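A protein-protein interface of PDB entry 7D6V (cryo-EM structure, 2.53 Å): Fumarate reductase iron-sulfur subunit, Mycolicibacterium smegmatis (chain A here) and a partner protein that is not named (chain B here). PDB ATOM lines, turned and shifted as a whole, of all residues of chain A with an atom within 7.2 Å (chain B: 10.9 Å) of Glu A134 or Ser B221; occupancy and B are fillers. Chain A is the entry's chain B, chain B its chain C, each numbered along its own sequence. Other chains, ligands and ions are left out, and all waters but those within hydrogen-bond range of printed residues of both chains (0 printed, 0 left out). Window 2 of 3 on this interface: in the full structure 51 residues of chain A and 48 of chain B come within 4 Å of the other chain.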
ATOM      1  N   MET A 131     -26.591 -23.028 -22.504  1.00  0.00           N
ATOM      2  CA  MET A 131     -26.771 -21.852 -21.668  1.00  0.00           C
ATOM      3  C   MET A 131     -27.969 -22.062 -20.759  1.00  0.00           C
ATOM      4  O   MET A 131     -29.005 -22.570 -21.195  1.00  0.00           O
ATOM      5  CB  MET A 131     -26.974 -20.586 -22.510  1.00  0.00           C
ATOM      6  CG  MET A 131     -25.832 -20.273 -23.459  1.00  0.00           C
ATOM      7  SD  MET A 131     -26.135 -18.814 -24.464  1.00  0.00           S
ATOM      8  CE  MET A 131     -27.016 -19.538 -25.838  1.00  0.00           C
ATOM      9  N   GLN A 132     -27.826 -21.673 -19.499  1.00  0.00           N
ATOM     10  CA  GLN A 132     -28.936 -21.693 -18.561  1.00  0.00           C
ATOM     11  C   GLN A 132     -29.733 -20.396 -18.663  1.00  0.00           C
ATOM     12  O   GLN A 132     -29.223 -19.358 -19.086  1.00  0.00           O
ATOM     13  CB  GLN A 132     -28.431 -21.905 -17.135  1.00  0.00           C
ATOM     14  CG  GLN A 132     -27.653 -23.198 -16.939  1.00  0.00           C
ATOM     15  CD  GLN A 132     -28.519 -24.434 -17.096  1.00  0.00           C
ATOM     16  OE1 GLN A 132     -29.682 -24.443 -16.702  1.00  0.00           O
ATOM     17  NE2 GLN A 132     -27.952 -25.484 -17.673  1.00  0.00           N
ATOM     18  N   GLN A 133     -31.007 -20.473 -18.271  1.00  0.00           N
ATOM     19  CA  GLN A 133     -31.907 -19.333 -18.426  1.00  0.00           C
ATOM     20  C   GLN A 133     -31.460 -18.140 -17.586  1.00  0.00           C
ATOM     21  O   GLN A 133     -31.495 -16.991 -18.052  1.00  0.00           O
ATOM     22  CB  GLN A 133     -33.331 -19.743 -18.059  1.00  0.00           C
ATOM     23  CG  GLN A 133     -34.360 -18.649 -18.245  1.00  0.00           C
ATOM     24  CD  GLN A 133     -34.581 -18.302 -19.699  1.00  0.00           C
ATOM     25  OE1 GLN A 133     -34.722 -19.181 -20.543  1.00  0.00           O
ATOM     26  NE2 GLN A 133     -34.618 -17.013 -20.000  1.00  0.00           N
ATOM     27  N   GLU A 134     -31.049 -18.390 -16.341  1.00  0.00           N
ATOM     28  CA  GLU A 134     -30.604 -17.303 -15.479  1.00  0.00           C
ATOM     29  C   GLU A 134     -29.332 -16.651 -15.992  1.00  0.00           C
ATOM     30  O   GLU A 134     -29.057 -15.499 -15.644  1.00  0.00           O
ATOM     31  CB  GLU A 134     -30.400 -17.810 -14.052  1.00  0.00           C
ATOM     32  CG  GLU A 134     -29.252 -18.781 -13.889  1.00  0.00           C
ATOM     33  CD  GLU A 134     -29.696 -20.223 -13.962  1.00  0.00           C
ATOM     34  OE1 GLU A 134     -30.762 -20.490 -14.556  1.00  0.00           O
ATOM     35  OE2 GLU A 134     -28.979 -21.093 -13.428  1.00  0.00           O
ATOM     36  N   ASP A 135     -28.557 -17.358 -16.815  1.00  0.00           N
ATOM     37  CA  ASP A 135     -27.372 -16.785 -17.433  1.00  0.00           C
ATOM     38  C   ASP A 135     -27.699 -15.907 -18.631  1.00  0.00           C
ATOM     39  O   ASP A 135     -26.845 -15.126 -19.058  1.00  0.00           O
ATOM     40  CB  ASP A 135     -26.416 -17.895 -17.869  1.00  0.00           C
ATOM     41  CG  ASP A 135     -25.721 -18.558 -16.704  1.00  0.00           C
ATOM     42  OD1 ASP A 135     -26.026 -18.207 -15.549  1.00  0.00           O
ATOM     43  OD2 ASP A 135     -24.865 -19.434 -16.945  1.00  0.00           O
ATOM     44  N   VAL A 136     -28.907 -16.013 -19.181  1.00  0.00           N
ATOM     45  CA  VAL A 136     -29.274 -15.276 -20.385  1.00  0.00           C
ATOM     46  C   VAL A 136     -30.370 -14.251 -20.152  1.00  0.00           C
ATOM     47  O   VAL A 136     -30.694 -13.504 -21.086  1.00  0.00           O
ATOM     48  CB  VAL A 136     -29.688 -16.228 -21.528  1.00  0.00           C
ATOM     49  CG1 VAL A 136     -28.658 -17.327 -21.704  1.00  0.00           C
ATOM     50  CG2 VAL A 136     -31.063 -16.814 -21.262  1.00  0.00           C
ATOM     51  N   ASN A 137     -30.958 -14.195 -18.953  1.00  0.00           N
ATOM     52  CA  ASN A 137     -32.066 -13.269 -18.710  1.00  0.00           C
ATOM     53  C   ASN A 137     -31.657 -11.812 -18.922  1.00  0.00           C
ATOM     54  O   ASN A 137     -32.399 -11.031 -19.537  1.00  0.00           O
ATOM     55  CB  ASN A 137     -32.601 -13.463 -17.292  1.00  0.00           C
ATOM     56  CG  ASN A 137     -33.541 -14.638 -17.178  1.00  0.00           C
ATOM     57  OD1 ASN A 137     -34.321 -14.910 -18.087  1.00  0.00           O
ATOM     58  ND2 ASN A 137     -33.476 -15.342 -16.058  1.00  0.00           N
ATOM     59  N   ARG A 138     -30.485 -11.426 -18.412  1.00  0.00           N
ATOM     60  CA  ARG A 138     -30.077 -10.026 -18.466  1.00  0.00           C
ATOM     61  C   ARG A 138     -29.905  -9.550 -19.902  1.00  0.00           C
ATOM     62  O   ARG A 138     -30.339  -8.449 -20.253  1.00  0.00           O
ATOM     63  CB  ARG A 138     -28.782  -9.825 -17.683  1.00  0.00           C
ATOM     64  CG  ARG A 138     -28.954  -9.862 -16.181  1.00  0.00           C
ATOM     65  CD  ARG A 138     -27.811  -9.152 -15.491  1.00  0.00           C
ATOM     66  NE  ARG A 138     -26.588  -9.943 -15.503  1.00  0.00           N
ATOM     67  CZ  ARG A 138     -25.456  -9.571 -14.919  1.00  0.00           C
ATOM     68  NH1 ARG A 138     -25.393  -8.417 -14.273  1.00  0.00           N
ATOM     69  NH2 ARG A 138     -24.389 -10.351 -14.978  1.00  0.00           N
ATOM     70  N   PRO A 184     -23.300 -15.060 -21.784  1.00  0.00           N
ATOM     71  CA  PRO A 184     -22.486 -16.077 -21.098  1.00  0.00           C
ATOM     72  C   PRO A 184     -21.427 -16.728 -21.971  1.00  0.00           C
ATOM     73  O   PRO A 184     -20.466 -17.284 -21.430  1.00  0.00           O
ATOM     74  CB  PRO A 184     -23.528 -17.101 -20.627  1.00  0.00           C
ATOM     75  CG  PRO A 184     -24.737 -16.840 -21.454  1.00  0.00           C
ATOM     76  CD  PRO A 184     -24.734 -15.386 -21.759  1.00  0.00           C
ATOM     77  N   GLY B 214     -23.476  -9.476  -6.791  1.00  0.00           N
ATOM     78  CA  GLY B 214     -23.414 -10.376  -7.924  1.00  0.00           C
ATOM     79  C   GLY B 214     -23.543  -9.721  -9.283  1.00  0.00           C
ATOM     80  O   GLY B 214     -23.607 -10.416 -10.299  1.00  0.00           O
ATOM     81  N   GLY B 215     -23.571  -8.390  -9.323  1.00  0.00           N
ATOM     82  CA  GLY B 215     -23.783  -7.704 -10.585  1.00  0.00           C
ATOM     83  C   GLY B 215     -22.643  -7.871 -11.566  1.00  0.00           C
ATOM     84  O   GLY B 215     -22.864  -7.905 -12.779  1.00  0.00           O
ATOM     85  N   LEU B 217     -20.772 -10.497 -11.946  1.00  0.00           N
ATOM     86  CA  LEU B 217     -20.569 -11.876 -12.357  1.00  0.00           C
ATOM     87  C   LEU B 217     -21.098 -12.098 -13.770  1.00  0.00           C
ATOM     88  O   LEU B 217     -21.940 -11.351 -14.273  1.00  0.00           O
ATOM     89  CB  LEU B 217     -21.258 -12.834 -11.385  1.00  0.00           C
ATOM     90  CG  LEU B 217     -20.604 -13.003 -10.014  1.00  0.00           C
ATOM     91  CD1 LEU B 217     -21.561 -13.662  -9.046  1.00  0.00           C
ATOM     92  CD2 LEU B 217     -19.325 -13.805 -10.124  1.00  0.00           C
ATOM     93  N   LYS B 218     -20.588 -13.146 -14.413  1.00  0.00           N
ATOM     94  CA  LYS B 218     -21.060 -13.550 -15.733  1.00  0.00           C
ATOM     95  C   LYS B 218     -22.002 -14.743 -15.676  1.00  0.00           C
ATOM     96  O   LYS B 218     -23.101 -14.693 -16.235  1.00  0.00           O
ATOM     97  CB  LYS B 218     -19.878 -13.871 -16.656  1.00  0.00           C
ATOM     98  CG  LYS B 218     -20.309 -14.263 -18.062  1.00  0.00           C
ATOM     99  CD  LYS B 218     -19.127 -14.565 -18.965  1.00  0.00           C
ATOM    100  CE  LYS B 218     -18.445 -13.300 -19.433  1.00  0.00           C
ATOM    101  NZ  LYS B 218     -19.309 -12.541 -20.373  1.00  0.00           N
ATOM    102  N   HIS B 219     -21.600 -15.818 -15.011  1.00  0.00           N
ATOM    103  CA  HIS B 219     -22.400 -17.033 -14.919  1.00  0.00           C
ATOM    104  C   HIS B 219     -23.061 -17.079 -13.545  1.00  0.00           C
ATOM    105  O   HIS B 219     -22.429 -17.444 -12.553  1.00  0.00           O
ATOM    106  CB  HIS B 219     -21.539 -18.266 -15.163  1.00  0.00           C
ATOM    107  N   PHE B 220     -24.342 -16.706 -13.497  1.00  0.00           N
ATOM    108  CA  PHE B 220     -25.115 -16.839 -12.270  1.00  0.00           C
ATOM    109  C   PHE B 220     -25.359 -18.294 -11.903  1.00  0.00           C
ATOM    110  O   PHE B 220     -25.707 -18.582 -10.754  1.00  0.00           O
ATOM    111  CB  PHE B 220     -26.456 -16.115 -12.410  1.00  0.00           C
ATOM    112  CG  PHE B 220     -26.373 -14.631 -12.200  1.00  0.00           C
ATOM    113  CD1 PHE B 220     -25.569 -14.102 -11.207  1.00  0.00           C
ATOM    114  CD2 PHE B 220     -27.104 -13.765 -12.993  1.00  0.00           C
ATOM    115  CE1 PHE B 220     -25.494 -12.740 -11.013  1.00  0.00           C
ATOM    116  CE2 PHE B 220     -27.034 -12.401 -12.802  1.00  0.00           C
ATOM    117  CZ  PHE B 220     -26.227 -11.888 -11.812  1.00  0.00           C
ATOM    118  N   SER B 221     -25.191 -19.215 -12.855  1.00  0.00           N
ATOM    119  CA  SER B 221     -25.514 -20.614 -12.607  1.00  0.00           C
ATOM    120  C   SER B 221     -24.495 -21.285 -11.699  1.00  0.00           C
ATOM    121  O   SER B 221     -24.839 -22.230 -10.980  1.00  0.00           O
ATOM    122  CB  SER B 221     -25.622 -21.363 -13.933  1.00  0.00           C
ATOM    123  OG  SER B 221     -24.432 -21.241 -14.689  1.00  0.00           O
ATOM    124  N   LYS B 222     -23.245 -20.826 -11.710  1.00  0.00           N
ATOM    125  CA  LYS B 222     -22.210 -21.406 -10.868  1.00  0.00           C
ATOM    126  C   LYS B 222     -22.009 -20.650  -9.563  1.00  0.00           C
ATOM    127  O   LYS B 222     -21.100 -20.987  -8.799  1.00  0.00           O
ATOM    128  CB  LYS B 222     -20.888 -21.501 -11.631  1.00  0.00           C
ATOM    129  CG  LYS B 222     -20.925 -22.437 -12.828  1.00  0.00           C
ATOM    130  CD  LYS B 222     -19.561 -22.546 -13.493  1.00  0.00           C
ATOM    131  CE  LYS B 222     -19.156 -21.283 -14.221  1.00  0.00           C
ATOM    132  NZ  LYS B 222     -20.048 -21.042 -15.381  1.00  0.00           N
ATOM    133  N   HIS B 223     -22.833 -19.645  -9.287  1.00  0.00           N
ATOM    134  CA  HIS B 223     -22.763 -18.868  -8.050  1.00  0.00           C
ATOM    135  C   HIS B 223     -24.168 -18.758  -7.478  1.00  0.00           C
ATOM    136  O   HIS B 223     -24.831 -17.722  -7.619  1.00  0.00           O
ATOM    137  CB  HIS B 223     -22.130 -17.502  -8.306  1.00  0.00           C
ATOM    138  CG  HIS B 223     -20.762 -17.584  -8.904  1.00  0.00           C
ATOM    139  ND1 HIS B 223     -20.499 -17.245 -10.213  1.00  0.00           N
ATOM    140  CD2 HIS B 223     -19.582 -17.980  -8.375  1.00  0.00           C
ATOM    141  CE1 HIS B 223     -19.216 -17.425 -10.463  1.00  0.00           C
ATOM    142  NE2 HIS B 223     -18.637 -17.870  -9.363  1.00  0.00           N
ATOM    143  N   PRO B 224     -24.659 -19.817  -6.829  1.00  0.00           N
ATOM    144  CA  PRO B 224     -26.061 -19.808  -6.375  1.00  0.00           C
ATOM    145  C   PRO B 224     -26.341 -18.823  -5.255  1.00  0.00           C
ATOM    146  O   PRO B 224     -27.421 -18.222  -5.230  1.00  0.00           O
ATOM    147  CB  PRO B 224     -26.289 -21.258  -5.918  1.00  0.00           C
ATOM    148  CG  PRO B 224     -25.129 -22.039  -6.452  1.00  0.00           C
ATOM    149  CD  PRO B 224     -23.990 -21.091  -6.530  1.00  0.00           C
ATOM    150  N   VAL B 225     -25.412 -18.652  -4.316  1.00  0.00           N
ATOM    151  CA  VAL B 225     -25.640 -17.744  -3.195  1.00  0.00           C
ATOM    152  C   VAL B 225     -25.669 -16.300  -3.676  1.00  0.00           C
ATOM    153  O   VAL B 225     -26.576 -15.526  -3.340  1.00  0.00           O
ATOM    154  CB  VAL B 225     -24.565 -17.957  -2.115  1.00  0.00           C
ATOM    155  CG1 VAL B 225     -24.713 -16.940  -1.004  1.00  0.00           C
ATOM    156  CG2 VAL B 225     -24.645 -19.366  -1.564  1.00  0.00           C
ATOM    157  N   ARG B 226     -24.683 -15.923  -4.489  1.00  0.00           N
ATOM    158  CA  ARG B 226     -24.600 -14.545  -4.947  1.00  0.00           C
ATOM    159  C   ARG B 226     -25.704 -14.219  -5.938  1.00  0.00           C
ATOM    160  O   ARG B 226     -26.118 -13.063  -6.031  1.00  0.00           O
ATOM    161  CB  ARG B 226     -23.221 -14.281  -5.545  1.00  0.00           C
ATOM    162  CG  ARG B 226     -22.111 -14.378  -4.517  1.00  0.00           C
ATOM    163  CD  ARG B 226     -20.743 -14.295  -5.148  1.00  0.00           C
ATOM    164  NE  ARG B 226     -20.448 -12.942  -5.600  1.00  0.00           N
ATOM    165  CZ  ARG B 226     -19.285 -12.568  -6.118  1.00  0.00           C
ATOM    166  NH1 ARG B 226     -18.303 -13.448  -6.246  1.00  0.00           N
ATOM    167  NH2 ARG B 226     -19.107 -11.315  -6.507  1.00  0.00           N
ATOM    168  N   TYR B 227     -26.221 -15.221  -6.654  1.00  0.00           N
ATOM    169  CA  TYR B 227     -27.388 -14.995  -7.502  1.00  0.00           C
ATOM    170  C   TYR B 227     -28.611 -14.621  -6.671  1.00  0.00           C
ATOM    171  O   TYR B 227     -29.345 -13.689  -7.017  1.00  0.00           O
ATOM    172  CB  TYR B 227     -27.671 -16.239  -8.342  1.00  0.00           C
ATOM    173  CG  TYR B 227     -28.860 -16.093  -9.262  1.00  0.00           C
ATOM    174  CD1 TYR B 227     -29.007 -14.972 -10.062  1.00  0.00           C
ATOM    175  CD2 TYR B 227     -29.835 -17.074  -9.327  1.00  0.00           C
ATOM    176  CE1 TYR B 227     -30.085 -14.833 -10.900  1.00  0.00           C
ATOM    177  CE2 TYR B 227     -30.918 -16.942 -10.164  1.00  0.00           C
ATOM    178  CZ  TYR B 227     -31.038 -15.820 -10.948  1.00  0.00           C
ATOM    179  OH  TYR B 227     -32.120 -15.683 -11.786  1.00  0.00           O
ATOM    180  N   TRP B 228     -28.845 -15.337  -5.571  1.00  0.00           N
ATOM    181  CA  TRP B 228     -29.962 -15.015  -4.690  1.00  0.00           C
ATOM    182  C   TRP B 228     -29.795 -13.628  -4.079  1.00  0.00           C
ATOM    183  O   TRP B 228     -30.748 -12.831  -4.030  1.00  0.00           O
ATOM    184  CB  TRP B 228     -30.070 -16.083  -3.600  1.00  0.00           C
ATOM    185  CG  TRP B 228     -31.254 -15.949  -2.700  1.00  0.00           C
ATOM    186  CD1 TRP B 228     -32.492 -16.483  -2.891  1.00  0.00           C
ATOM    187  CD2 TRP B 228     -31.309 -15.242  -1.457  1.00  0.00           C
ATOM    188  NE1 TRP B 228     -33.318 -16.148  -1.849  1.00  0.00           N
ATOM    189  CE2 TRP B 228     -32.617 -15.383  -0.955  1.00  0.00           C
ATOM    190  CE3 TRP B 228     -30.384 -14.493  -0.724  1.00  0.00           C
ATOM    191  CZ2 TRP B 228     -33.021 -14.810   0.246  1.00  0.00           C
ATOM    192  CZ3 TRP B 228     -30.786 -13.928   0.467  1.00  0.00           C
ATOM    193  CH2 TRP B 228     -32.093 -14.088   0.941  1.00  0.00           C
ATOM    194  N   TRP B 230     -28.103 -11.136  -5.328  1.00  0.00           N
ATOM    195  CA  TRP B 230     -28.282 -10.154  -6.387  1.00  0.00           C
ATOM    196  C   TRP B 230     -29.754  -9.964  -6.725  1.00  0.00           C
ATOM    197  O   TRP B 230     -30.193  -8.843  -6.993  1.00  0.00           O
ATOM    198  CB  TRP B 230     -27.487 -10.582  -7.620  1.00  0.00           C
ATOM    199  CG  TRP B 230     -27.620  -9.659  -8.780  1.00  0.00           C
ATOM    200  CD1 TRP B 230     -26.941  -8.498  -8.984  1.00  0.00           C
ATOM    201  CD2 TRP B 230     -28.489  -9.818  -9.902  1.00  0.00           C
ATOM    202  NE1 TRP B 230     -27.332  -7.923 -10.164  1.00  0.00           N
ATOM    203  CE2 TRP B 230     -28.285  -8.715 -10.748  1.00  0.00           C
ATOM    204  CE3 TRP B 230     -29.424 -10.789 -10.275  1.00  0.00           C
ATOM    205  CZ2 TRP B 230     -28.977  -8.555 -11.941  1.00  0.00           C
ATOM    206  CZ3 TRP B 230     -30.108 -10.626 -11.457  1.00  0.00           C
ATOM    207  CH2 TRP B 230     -29.882  -9.519 -12.277  1.00  0.00           C
ATOM    208  N   THR B 231     -30.534 -11.046  -6.716  1.00  0.00           N
ATOM    209  CA  THR B 231     -31.961 -10.930  -7.004  1.00  0.00           C
ATOM    210  C   THR B 231     -32.667 -10.069  -5.962  1.00  0.00           C
ATOM    211  O   THR B 231     -33.431  -9.153  -6.302  1.00  0.00           O
ATOM    212  CB  THR B 231     -32.591 -12.321  -7.069  1.00  0.00           C
ATOM    213  OG1 THR B 231     -32.002 -13.061  -8.144  1.00  0.00           O
ATOM    214  CG2 THR B 231     -34.087 -12.219  -7.297  1.00  0.00           C
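The side-chain carboxylate (OD1) of Asp A135 lies within hydrogen-bond range of the backbone NH (N) of Phe B220 (3.0 Å).
OG of Ser B221 sits at hydrogen-bond distance from OD2 of Asp A135, at 2.9 Å.
O of Gly B215 sits at hydrogen-bond distance from NH1 of Arg A138.
NH2 of Arg A138 lies within hydrogen-bond range of O of Leu B217 (2.7 Å).
The backbone carbonyl oxygen (O) of His B219 lies within hydrogen-bond range of a ring nitrogen (ND1) of His B223 (3.0 Å).
OG1 of Thr B231 lies within hydrogen-bond range of O of Tyr B227 (3.0 Å).
CD2 of Phe B220 touches O of Glu A134 (3.7 Å).
CB of Ser B221 touches OE2 of Glu A134 (3.4 Å).
OH of Tyr B227 touches CB of Glu A134, 3.6 Å away.
OD1 of Asp A135 touches C of His B219 (3.8 Å).
NE of Arg A138 touches CE2 of Phe B220 (3.7 Å).
Trp B230 touches Arg A138.
O of Pro A184 touches CD of Lys B218, at 3.9 Å.
Of chain B, only Phe B220 (3.7 Å), Ser B221 (3.4 Å) and Tyr B227 (3.6 Å) come within 4 Å of Glu A134.
Ser B221 touches just these residues of chain A: Glu A134 and Asp A135.
No residue of chain B comes within 4 Å of Gln A132.
No residue of chain B comes within 4 Å of Gln A133.
Of the printed residues of chain B, Asp A135 touches His B219, Phe B220 and Ser B221.
No residue of chain B comes within 4 Å of Val A136.
No residue of chain B comes within 4 Å of Asn A137.
Printed residues of chain A within 4 Å of Lys B218: Pro A184 (3.9 Å).
Of the printed residues of chain A, Tyr B227 touches Glu A134.
The nearest residue of chain B that does not touch Glu A134 is Lys B222 (6.0 Å).
Of the 9 printed residues of chain A, 4 touch a printed residue of chain B.
Among the printed residues, no Asp or Glu carboxylate lies within 4 Å of a Lys or Arg side-chain nitrogen of the other chain.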
